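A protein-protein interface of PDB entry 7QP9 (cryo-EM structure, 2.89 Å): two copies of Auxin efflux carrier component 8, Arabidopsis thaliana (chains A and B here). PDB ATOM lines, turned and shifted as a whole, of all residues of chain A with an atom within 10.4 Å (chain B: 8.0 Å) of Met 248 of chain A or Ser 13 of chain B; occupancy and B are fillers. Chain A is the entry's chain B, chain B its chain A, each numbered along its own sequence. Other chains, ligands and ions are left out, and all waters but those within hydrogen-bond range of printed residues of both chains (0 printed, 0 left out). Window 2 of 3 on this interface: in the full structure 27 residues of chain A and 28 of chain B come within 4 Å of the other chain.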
ATOM      1  N   PHE A  57      24.951 -28.006 -30.533  1.00  0.00           N
ATOM      2  CA  PHE A  57      24.267 -29.221 -30.105  1.00  0.00           C
ATOM      3  C   PHE A  57      22.773 -29.128 -30.374  1.00  0.00           C
ATOM      4  O   PHE A  57      22.159 -30.089 -30.850  1.00  0.00           O
ATOM      5  CB  PHE A  57      24.509 -29.492 -28.622  1.00  0.00           C
ATOM      6  CG  PHE A  57      23.615 -30.561 -28.065  1.00  0.00           C
ATOM      7  CD1 PHE A  57      23.900 -31.899 -28.277  1.00  0.00           C
ATOM      8  CD2 PHE A  57      22.476 -30.233 -27.354  1.00  0.00           C
ATOM      9  CE1 PHE A  57      23.074 -32.884 -27.780  1.00  0.00           C
ATOM     10  CE2 PHE A  57      21.647 -31.216 -26.857  1.00  0.00           C
ATOM     11  CZ  PHE A  57      21.947 -32.542 -27.071  1.00  0.00           C
ATOM     12  N   ASN A 244      13.621 -39.508 -26.214  1.00  0.00           N
ATOM     13  CA  ASN A 244      13.350 -38.090 -26.034  1.00  0.00           C
ATOM     14  C   ASN A 244      14.277 -37.526 -24.968  1.00  0.00           C
ATOM     15  O   ASN A 244      14.495 -38.152 -23.927  1.00  0.00           O
ATOM     16  CB  ASN A 244      11.891 -37.855 -25.637  1.00  0.00           C
ATOM     17  CG  ASN A 244      11.023 -37.464 -26.815  1.00  0.00           C
ATOM     18  OD1 ASN A 244      11.287 -36.471 -27.492  1.00  0.00           O
ATOM     19  ND2 ASN A 244       9.980 -38.245 -27.066  1.00  0.00           N
ATOM     20  N   LEU A 245      14.820 -36.348 -25.234  1.00  0.00           N
ATOM     21  CA  LEU A 245      15.753 -35.735 -24.299  1.00  0.00           C
ATOM     22  C   LEU A 245      15.021 -35.371 -23.013  1.00  0.00           C
ATOM     23  O   LEU A 245      13.970 -34.722 -23.071  1.00  0.00           O
ATOM     24  CB  LEU A 245      16.386 -34.494 -24.924  1.00  0.00           C
ATOM     25  CG  LEU A 245      17.623 -33.909 -24.243  1.00  0.00           C
ATOM     26  CD1 LEU A 245      18.771 -34.899 -24.227  1.00  0.00           C
ATOM     27  CD2 LEU A 245      18.040 -32.631 -24.943  1.00  0.00           C
ATOM     28  N   PRO A 246      15.528 -35.762 -21.843  1.00  0.00           N
ATOM     29  CA  PRO A 246      14.830 -35.421 -20.599  1.00  0.00           C
ATOM     30  C   PRO A 246      14.607 -33.921 -20.485  1.00  0.00           C
ATOM     31  O   PRO A 246      15.470 -33.116 -20.838  1.00  0.00           O
ATOM     32  CB  PRO A 246      15.771 -35.940 -19.508  1.00  0.00           C
ATOM     33  CG  PRO A 246      16.540 -37.022 -20.157  1.00  0.00           C
ATOM     34  CD  PRO A 246      16.683 -36.644 -21.599  1.00  0.00           C
ATOM     35  N   GLU A 247      13.429 -33.554 -19.983  1.00  0.00           N
ATOM     36  CA  GLU A 247      13.052 -32.146 -19.932  1.00  0.00           C
ATOM     37  C   GLU A 247      14.064 -31.330 -19.137  1.00  0.00           C
ATOM     38  O   GLU A 247      14.350 -30.175 -19.479  1.00  0.00           O
ATOM     39  CB  GLU A 247      11.659 -32.006 -19.324  1.00  0.00           C
ATOM     40  CG  GLU A 247      11.039 -30.645 -19.533  1.00  0.00           C
ATOM     41  CD  GLU A 247       9.743 -30.468 -18.770  1.00  0.00           C
ATOM     42  OE1 GLU A 247       9.430 -31.328 -17.919  1.00  0.00           O
ATOM     43  OE2 GLU A 247       9.035 -29.470 -19.020  1.00  0.00           O
ATOM     44  N   MET A 248      14.618 -31.913 -18.072  1.00  0.00           N
ATOM     45  CA  MET A 248      15.602 -31.195 -17.269  1.00  0.00           C
ATOM     46  C   MET A 248      16.817 -30.816 -18.101  1.00  0.00           C
ATOM     47  O   MET A 248      17.300 -29.683 -18.027  1.00  0.00           O
ATOM     48  CB  MET A 248      16.029 -32.051 -16.077  1.00  0.00           C
ATOM     49  CG  MET A 248      14.931 -32.302 -15.070  1.00  0.00           C
ATOM     50  SD  MET A 248      15.505 -33.260 -13.658  1.00  0.00           S
ATOM     51  CE  MET A 248      15.646 -34.884 -14.393  1.00  0.00           C
ATOM     52  N   ILE A 249      17.323 -31.753 -18.905  1.00  0.00           N
ATOM     53  CA  ILE A 249      18.507 -31.481 -19.714  1.00  0.00           C
ATOM     54  C   ILE A 249      18.194 -30.446 -20.789  1.00  0.00           C
ATOM     55  O   ILE A 249      19.012 -29.565 -21.079  1.00  0.00           O
ATOM     56  CB  ILE A 249      19.046 -32.788 -20.321  1.00  0.00           C
ATOM     57  CG1 ILE A 249      19.423 -33.769 -19.210  1.00  0.00           C
ATOM     58  CG2 ILE A 249      20.245 -32.503 -21.206  1.00  0.00           C
ATOM     59  CD1 ILE A 249      19.729 -35.161 -19.697  1.00  0.00           C
ATOM     60  N   ASP A 250      17.015 -30.541 -21.403  1.00  0.00           N
ATOM     61  CA  ASP A 250      16.632 -29.568 -22.419  1.00  0.00           C
ATOM     62  C   ASP A 250      16.570 -28.163 -21.833  1.00  0.00           C
ATOM     63  O   ASP A 250      17.099 -27.208 -22.415  1.00  0.00           O
ATOM     64  CB  ASP A 250      15.285 -29.960 -23.028  1.00  0.00           C
ATOM     65  CG  ASP A 250      15.077 -29.381 -24.412  1.00  0.00           C
ATOM     66  OD1 ASP A 250      16.052 -28.880 -25.009  1.00  0.00           O
ATOM     67  OD2 ASP A 250      13.930 -29.426 -24.905  1.00  0.00           O
ATOM     68  N   LYS A 251      15.932 -28.019 -20.669  1.00  0.00           N
ATOM     69  CA  LYS A 251      15.876 -26.712 -20.023  1.00  0.00           C
ATOM     70  C   LYS A 251      17.261 -26.237 -19.608  1.00  0.00           C
ATOM     71  O   LYS A 251      17.570 -25.047 -19.716  1.00  0.00           O
ATOM     72  CB  LYS A 251      14.941 -26.752 -18.814  1.00  0.00           C
ATOM     73  CG  LYS A 251      13.477 -26.957 -19.160  1.00  0.00           C
ATOM     74  CD  LYS A 251      12.615 -26.928 -17.910  1.00  0.00           C
ATOM     75  CE  LYS A 251      11.158 -27.207 -18.229  1.00  0.00           C
ATOM     76  NZ  LYS A 251      10.547 -26.107 -19.026  1.00  0.00           N
ATOM     77  N   SER A 252      18.108 -27.146 -19.123  1.00  0.00           N
ATOM     78  CA  SER A 252      19.458 -26.755 -18.734  1.00  0.00           C
ATOM     79  C   SER A 252      20.230 -26.204 -19.922  1.00  0.00           C
ATOM     80  O   SER A 252      20.927 -25.189 -19.806  1.00  0.00           O
ATOM     81  CB  SER A 252      20.195 -27.950 -18.131  1.00  0.00           C
ATOM     82  OG  SER A 252      19.433 -28.554 -17.103  1.00  0.00           O
ATOM     83  N   ILE A 253      20.122 -26.864 -21.075  1.00  0.00           N
ATOM     84  CA  ILE A 253      20.813 -26.390 -22.270  1.00  0.00           C
ATOM     85  C   ILE A 253      20.247 -25.050 -22.721  1.00  0.00           C
ATOM     86  O   ILE A 253      20.998 -24.127 -23.058  1.00  0.00           O
ATOM     87  CB  ILE A 253      20.726 -27.447 -23.383  1.00  0.00           C
ATOM     88  CG1 ILE A 253      21.566 -28.669 -23.015  1.00  0.00           C
ATOM     89  CG2 ILE A 253      21.192 -26.867 -24.704  1.00  0.00           C
ATOM     90  CD1 ILE A 253      21.027 -29.959 -23.570  1.00  0.00           C
ATOM     91  N   HIS A 254      18.918 -24.918 -22.734  1.00  0.00           N
ATOM     92  CA  HIS A 254      18.310 -23.677 -23.204  1.00  0.00           C
ATOM     93  C   HIS A 254      18.598 -22.514 -22.265  1.00  0.00           C
ATOM     94  O   HIS A 254      18.613 -21.358 -22.702  1.00  0.00           O
ATOM     95  CB  HIS A 254      16.803 -23.861 -23.367  1.00  0.00           C
ATOM     96  CG  HIS A 254      16.411 -24.473 -24.673  1.00  0.00           C
ATOM     97  ND1 HIS A 254      16.173 -25.822 -24.821  1.00  0.00           N
ATOM     98  CD2 HIS A 254      16.220 -23.923 -25.896  1.00  0.00           C
ATOM     99  CE1 HIS A 254      15.849 -26.075 -26.076  1.00  0.00           C
ATOM    100  NE2 HIS A 254      15.871 -24.939 -26.750  1.00  0.00           N
ATOM    101  N   LEU A 255      18.823 -22.789 -20.981  1.00  0.00           N
ATOM    102  CA  LEU A 255      19.079 -21.712 -20.031  1.00  0.00           C
ATOM    103  C   LEU A 255      20.354 -20.959 -20.383  1.00  0.00           C
ATOM    104  O   LEU A 255      20.403 -19.728 -20.294  1.00  0.00           O
ATOM    105  CB  LEU A 255      19.162 -22.279 -18.614  1.00  0.00           C
ATOM    106  CG  LEU A 255      18.812 -21.325 -17.472  1.00  0.00           C
ATOM    107  CD1 LEU A 255      17.328 -21.013 -17.472  1.00  0.00           C
ATOM    108  CD2 LEU A 255      19.230 -21.910 -16.138  1.00  0.00           C
ATOM    109  N   LEU A 256      21.397 -21.682 -20.788  1.00  0.00           N
ATOM    110  CA  LEU A 256      22.680 -21.073 -21.107  1.00  0.00           C
ATOM    111  C   LEU A 256      22.861 -20.776 -22.590  1.00  0.00           C
ATOM    112  O   LEU A 256      23.668 -19.906 -22.933  1.00  0.00           O
ATOM    113  CB  LEU A 256      23.826 -21.982 -20.647  1.00  0.00           C
ATOM    114  CG  LEU A 256      24.379 -21.713 -19.247  1.00  0.00           C
ATOM    115  CD1 LEU A 256      25.286 -22.850 -18.817  1.00  0.00           C
ATOM    116  CD2 LEU A 256      25.122 -20.390 -19.197  1.00  0.00           C
ATOM    117  N   LEU B   6       4.148 -36.053  -8.998  1.00  0.00           N
ATOM    118  CA  LEU B   6       4.386 -35.452 -10.304  1.00  0.00           C
ATOM    119  C   LEU B   6       4.691 -33.965 -10.210  1.00  0.00           C
ATOM    120  O   LEU B   6       5.447 -33.443 -11.037  1.00  0.00           O
ATOM    121  CB  LEU B   6       3.175 -35.671 -11.214  1.00  0.00           C
ATOM    122  CG  LEU B   6       3.285 -35.109 -12.635  1.00  0.00           C
ATOM    123  CD1 LEU B   6       4.551 -35.597 -13.322  1.00  0.00           C
ATOM    124  CD2 LEU B   6       2.057 -35.483 -13.448  1.00  0.00           C
ATOM    125  N   ASP B   7       4.114 -33.269  -9.228  1.00  0.00           N
ATOM    126  CA  ASP B   7       4.454 -31.866  -9.014  1.00  0.00           C
ATOM    127  C   ASP B   7       5.808 -31.712  -8.334  1.00  0.00           C
ATOM    128  O   ASP B   7       6.501 -30.715  -8.564  1.00  0.00           O
ATOM    129  CB  ASP B   7       3.366 -31.177  -8.187  1.00  0.00           C
ATOM    130  CG  ASP B   7       3.065 -31.904  -6.894  1.00  0.00           C
ATOM    131  OD1 ASP B   7       4.006 -32.138  -6.107  1.00  0.00           O
ATOM    132  OD2 ASP B   7       1.887 -32.245  -6.665  1.00  0.00           O
ATOM    133  N   ILE B   8       6.198 -32.676  -7.497  1.00  0.00           N
ATOM    134  CA  ILE B   8       7.554 -32.673  -6.957  1.00  0.00           C
ATOM    135  C   ILE B   8       8.563 -32.765  -8.093  1.00  0.00           C
ATOM    136  O   ILE B   8       9.607 -32.101  -8.075  1.00  0.00           O
ATOM    137  CB  ILE B   8       7.732 -33.819  -5.944  1.00  0.00           C
ATOM    138  CG1 ILE B   8       6.799 -33.619  -4.748  1.00  0.00           C
ATOM    139  CG2 ILE B   8       9.179 -33.901  -5.481  1.00  0.00           C
ATOM    140  CD1 ILE B   8       6.711 -34.819  -3.827  1.00  0.00           C
ATOM    141  N   TYR B   9       8.269 -33.591  -9.098  1.00  0.00           N
ATOM    142  CA  TYR B   9       9.136 -33.656 -10.266  1.00  0.00           C
ATOM    143  C   TYR B   9       9.163 -32.326 -11.003  1.00  0.00           C
ATOM    144  O   TYR B   9      10.197 -31.935 -11.547  1.00  0.00           O
ATOM    145  CB  TYR B   9       8.686 -34.772 -11.206  1.00  0.00           C
ATOM    146  CG  TYR B   9       9.389 -34.732 -12.542  1.00  0.00           C
ATOM    147  CD1 TYR B   9      10.704 -35.156 -12.667  1.00  0.00           C
ATOM    148  CD2 TYR B   9       8.745 -34.257 -13.676  1.00  0.00           C
ATOM    149  CE1 TYR B   9      11.355 -35.115 -13.883  1.00  0.00           C
ATOM    150  CE2 TYR B   9       9.387 -34.213 -14.895  1.00  0.00           C
ATOM    151  CZ  TYR B   9      10.692 -34.643 -14.994  1.00  0.00           C
ATOM    152  OH  TYR B   9      11.337 -34.602 -16.209  1.00  0.00           O
ATOM    153  N   HIS B  10       8.031 -31.618 -11.041  1.00  0.00           N
ATOM    154  CA  HIS B  10       8.014 -30.305 -11.680  1.00  0.00           C
ATOM    155  C   HIS B  10       8.898 -29.317 -10.929  1.00  0.00           C
ATOM    156  O   HIS B  10       9.633 -28.534 -11.543  1.00  0.00           O
ATOM    157  CB  HIS B  10       6.579 -29.786 -11.770  1.00  0.00           C
ATOM    158  CG  HIS B  10       5.748 -30.486 -12.799  1.00  0.00           C
ATOM    159  ND1 HIS B  10       4.469 -30.932 -12.545  1.00  0.00           N
ATOM    160  CD2 HIS B  10       6.014 -30.818 -14.084  1.00  0.00           C
ATOM    161  CE1 HIS B  10       3.982 -31.509 -13.629  1.00  0.00           C
ATOM    162  NE2 HIS B  10       4.900 -31.453 -14.577  1.00  0.00           N
ATOM    163  N   VAL B  11       8.844 -29.341  -9.596  1.00  0.00           N
ATOM    164  CA  VAL B  11       9.714 -28.478  -8.802  1.00  0.00           C
ATOM    165  C   VAL B  11      11.176 -28.819  -9.061  1.00  0.00           C
ATOM    166  O   VAL B  11      12.019 -27.930  -9.239  1.00  0.00           O
ATOM    167  CB  VAL B  11       9.363 -28.603  -7.308  1.00  0.00           C
ATOM    168  CG1 VAL B  11      10.323 -27.782  -6.459  1.00  0.00           C
ATOM    169  CG2 VAL B  11       7.929 -28.176  -7.063  1.00  0.00           C
ATOM    170  N   VAL B  12      11.499 -30.113  -9.080  1.00  0.00           N
ATOM    171  CA  VAL B  12      12.877 -30.534  -9.315  1.00  0.00           C
ATOM    172  C   VAL B  12      13.333 -30.109 -10.704  1.00  0.00           C
ATOM    173  O   VAL B  12      14.484 -29.703 -10.897  1.00  0.00           O
ATOM    174  CB  VAL B  12      13.009 -32.054  -9.114  1.00  0.00           C
ATOM    175  CG1 VAL B  12      14.410 -32.522  -9.472  1.00  0.00           C
ATOM    176  CG2 VAL B  12      12.666 -32.430  -7.680  1.00  0.00           C
ATOM    177  N   SER B  13      12.446 -30.205 -11.694  1.00  0.00           N
ATOM    178  CA  SER B  13      12.798 -29.811 -13.053  1.00  0.00           C
ATOM    179  C   SER B  13      12.992 -28.308 -13.168  1.00  0.00           C
ATOM    180  O   SER B  13      13.809 -27.850 -13.973  1.00  0.00           O
ATOM    181  CB  SER B  13      11.721 -30.276 -14.031  1.00  0.00           C
ATOM    182  OG  SER B  13      11.466 -31.662 -13.890  1.00  0.00           O
ATOM    183  N   ALA B  14      12.235 -27.527 -12.398  1.00  0.00           N
ATOM    184  CA  ALA B  14      12.453 -26.085 -12.383  1.00  0.00           C
ATOM    185  C   ALA B  14      13.774 -25.737 -11.711  1.00  0.00           C
ATOM    186  O   ALA B  14      14.469 -24.808 -12.137  1.00  0.00           O
ATOM    187  CB  ALA B  14      11.293 -25.388 -11.676  1.00  0.00           C
ATOM    188  N   THR B  15      14.133 -26.467 -10.654  1.00  0.00           N
ATOM    189  CA  THR B  15      15.336 -26.144  -9.895  1.00  0.00           C
ATOM    190  C   THR B  15      16.611 -26.603 -10.599  1.00  0.00           C
ATOM    191  O   THR B  15      17.643 -25.932 -10.510  1.00  0.00           O
ATOM    192  CB  THR B  15      15.252 -26.772  -8.502  1.00  0.00           C
ATOM    193  OG1 THR B  15      14.229 -26.119  -7.742  1.00  0.00           O
ATOM    194  CG2 THR B  15      16.579 -26.647  -7.770  1.00  0.00           C
ATOM    195  N   VAL B  16      16.565 -27.743 -11.296  1.00  0.00           N
ATOM    196  CA  VAL B  16      17.801 -28.359 -11.789  1.00  0.00           C
ATOM    197  C   VAL B  16      18.525 -27.485 -12.801  1.00  0.00           C
ATOM    198  O   VAL B  16      19.755 -27.376 -12.716  1.00  0.00           O
ATOM    199  CB  VAL B  16      17.511 -29.771 -12.317  1.00  0.00           C
ATOM    200  CG1 VAL B  16      18.643 -30.249 -13.213  1.00  0.00           C
ATOM    201  CG2 VAL B  16      17.318 -30.730 -11.158  1.00  0.00           C
ATOM    202  N   PRO B  17      17.868 -26.882 -13.795  1.00  0.00           N
ATOM    203  CA  PRO B  17      18.624 -26.070 -14.767  1.00  0.00           C
ATOM    204  C   PRO B  17      19.459 -24.978 -14.119  1.00  0.00           C
ATOM    205  O   PRO B  17      20.596 -24.717 -14.545  1.00  0.00           O
ATOM    206  CB  PRO B  17      17.520 -25.490 -15.660  1.00  0.00           C
ATOM    207  CG  PRO B  17      16.399 -26.457 -15.559  1.00  0.00           C
ATOM    208  CD  PRO B  17      16.462 -27.055 -14.188  1.00  0.00           C
ATOM    209  N   LEU B  18      18.922 -24.333 -13.082  1.00  0.00           N
ATOM    210  CA  LEU B  18      19.681 -23.303 -12.387  1.00  0.00           C
ATOM    211  C   LEU B  18      20.934 -23.884 -11.754  1.00  0.00           C
ATOM    212  O   LEU B  18      22.023 -23.319 -11.890  1.00  0.00           O
ATOM    213  CB  LEU B  18      18.810 -22.634 -11.325  1.00  0.00           C
ATOM    214  CG  LEU B  18      17.379 -22.280 -11.723  1.00  0.00           C
ATOM    215  CD1 LEU B  18      16.753 -21.423 -10.646  1.00  0.00           C
ATOM    216  CD2 LEU B  18      17.355 -21.562 -13.057  1.00  0.00           C
ATOM    217  N   VAL B  20      22.488 -26.494 -12.695  1.00  0.00           N
ATOM    218  CA  VAL B  20      23.388 -26.922 -13.760  1.00  0.00           C
ATOM    219  C   VAL B  20      24.225 -25.747 -14.245  1.00  0.00           C
ATOM    220  O   VAL B  20      25.442 -25.867 -14.433  1.00  0.00           O
ATOM    221  CB  VAL B  20      22.589 -27.567 -14.906  1.00  0.00           C
ATOM    222  CG1 VAL B  20      23.446 -27.697 -16.155  1.00  0.00           C
ATOM    223  CG2 VAL B  20      22.060 -28.924 -14.473  1.00  0.00           C
ATOM    224  N   ILE B 121      10.459 -18.927 -11.385  1.00  0.00           N
ATOM    225  CA  ILE B 121      11.036 -20.188 -11.844  1.00  0.00           C
ATOM    226  C   ILE B 121      10.682 -21.311 -10.876  1.00  0.00           C
ATOM    227  O   ILE B 121      10.275 -22.403 -11.289  1.00  0.00           O
ATOM    228  CB  ILE B 121      12.558 -20.053 -12.023  1.00  0.00           C
ATOM    229  CG1 ILE B 121      12.877 -18.965 -13.049  1.00  0.00           C
ATOM    230  CG2 ILE B 121      13.158 -21.362 -12.516  1.00  0.00           C
ATOM    231  CD1 ILE B 121      13.081 -17.588 -12.452  1.00  0.00           C
ATOM    232  N   LEU B 122      10.819 -21.055  -9.577  1.00  0.00           N
ATOM    233  CA  LEU B 122      10.576 -22.069  -8.561  1.00  0.00           C
ATOM    234  C   LEU B 122       9.238 -21.902  -7.853  1.00  0.00           C
ATOM    235  O   LEU B 122       8.789 -22.844  -7.191  1.00  0.00           O
ATOM    236  CB  LEU B 122      11.702 -22.053  -7.519  1.00  0.00           C
ATOM    237  CG  LEU B 122      13.015 -22.717  -7.941  1.00  0.00           C
ATOM    238  CD1 LEU B 122      13.744 -21.882  -8.979  1.00  0.00           C
ATOM    239  CD2 LEU B 122      13.910 -22.961  -6.740  1.00  0.00           C
ATOM    240  N   PRO B 125       5.799 -23.831 -10.258  1.00  0.00           N
ATOM    241  CA  PRO B 125       5.481 -25.268 -10.317  1.00  0.00           C
ATOM    242  C   PRO B 125       4.791 -25.795  -9.073  1.00  0.00           C
ATOM    243  O   PRO B 125       3.958 -26.703  -9.178  1.00  0.00           O
ATOM    244  CB  PRO B 125       6.855 -25.925 -10.519  1.00  0.00           C
ATOM    245  CG  PRO B 125       7.753 -24.837 -10.992  1.00  0.00           C
ATOM    246  CD  PRO B 125       7.249 -23.592 -10.352  1.00  0.00           C
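Met 248 of chain A touches Ser 13 of chain B (CG to OG, 3.7 Å). Met 248 of chain A touches Val 16 of chain B (SD to CG2, 3.99 Å). Pro 17 of chain B touches Lys 251 of chain A. Pro 17 of chain B touches Ser 252 of chain A (CA to OG, 3.5 Å). Val 20 of chain B touches Ser 252 of chain A (CG2 to OG, 3.7 Å). Pro 17 of chain B touches Leu 255 of chain A (O to CD2, 3.5 Å). Leu 255 of chain A touches Leu 18 of chain B (CD2 to CD2, 3.6 Å).
Of the printed residues of chain B, Met 248 of chain A touches Ser 13 and Val 16. Of the printed residues of chain B, Leu 255 of chain A touches Pro 17 (3.5 Å) and Leu 18 (3.6 Å). Asp 7 of chain B touches none of the printed residues of chain A. No residue of chain A comes within 4 Å of Tyr 9 of chain B. No residue of chain A comes within 4 Å of Val 12 of chain B. Ser 13 of chain B touches one residue of chain A. No residue of chain A comes within 4 Å of Ala 14 of chain B. Printed residues of chain A within 4 Å of Val 20 of chain B: Ser 252 (3.7 Å). The nearest printed residue of chain B that does not touch Ser 252 of chain A is Val 16 of chain B (4.3 Å).
NZ of Lys 251 of chain A lies within salt-bridge range of OE2 of Glu 247 of chain A. OG of Ser 252 of chain A lies within hydrogen-bond range of O of Met 248 of chain A (2.6 Å). OG of Ser 13 of chain B is in hydrogen-bond range of O of Tyr 9 of chain B, at 2.7 Å.
Hydrophobic or aromatic side chains of chain B within 4 Å of the printed part of chain A: Val 16, Pro 17, Leu 18 and Val 20. Of the 14 printed residues of chain A, 4 touch a printed residue of chain B.
No position is printed for both chains. Of the 7 pairs that touch across the chains among the printed residues, none has its exchanged pair printed and touching as well.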
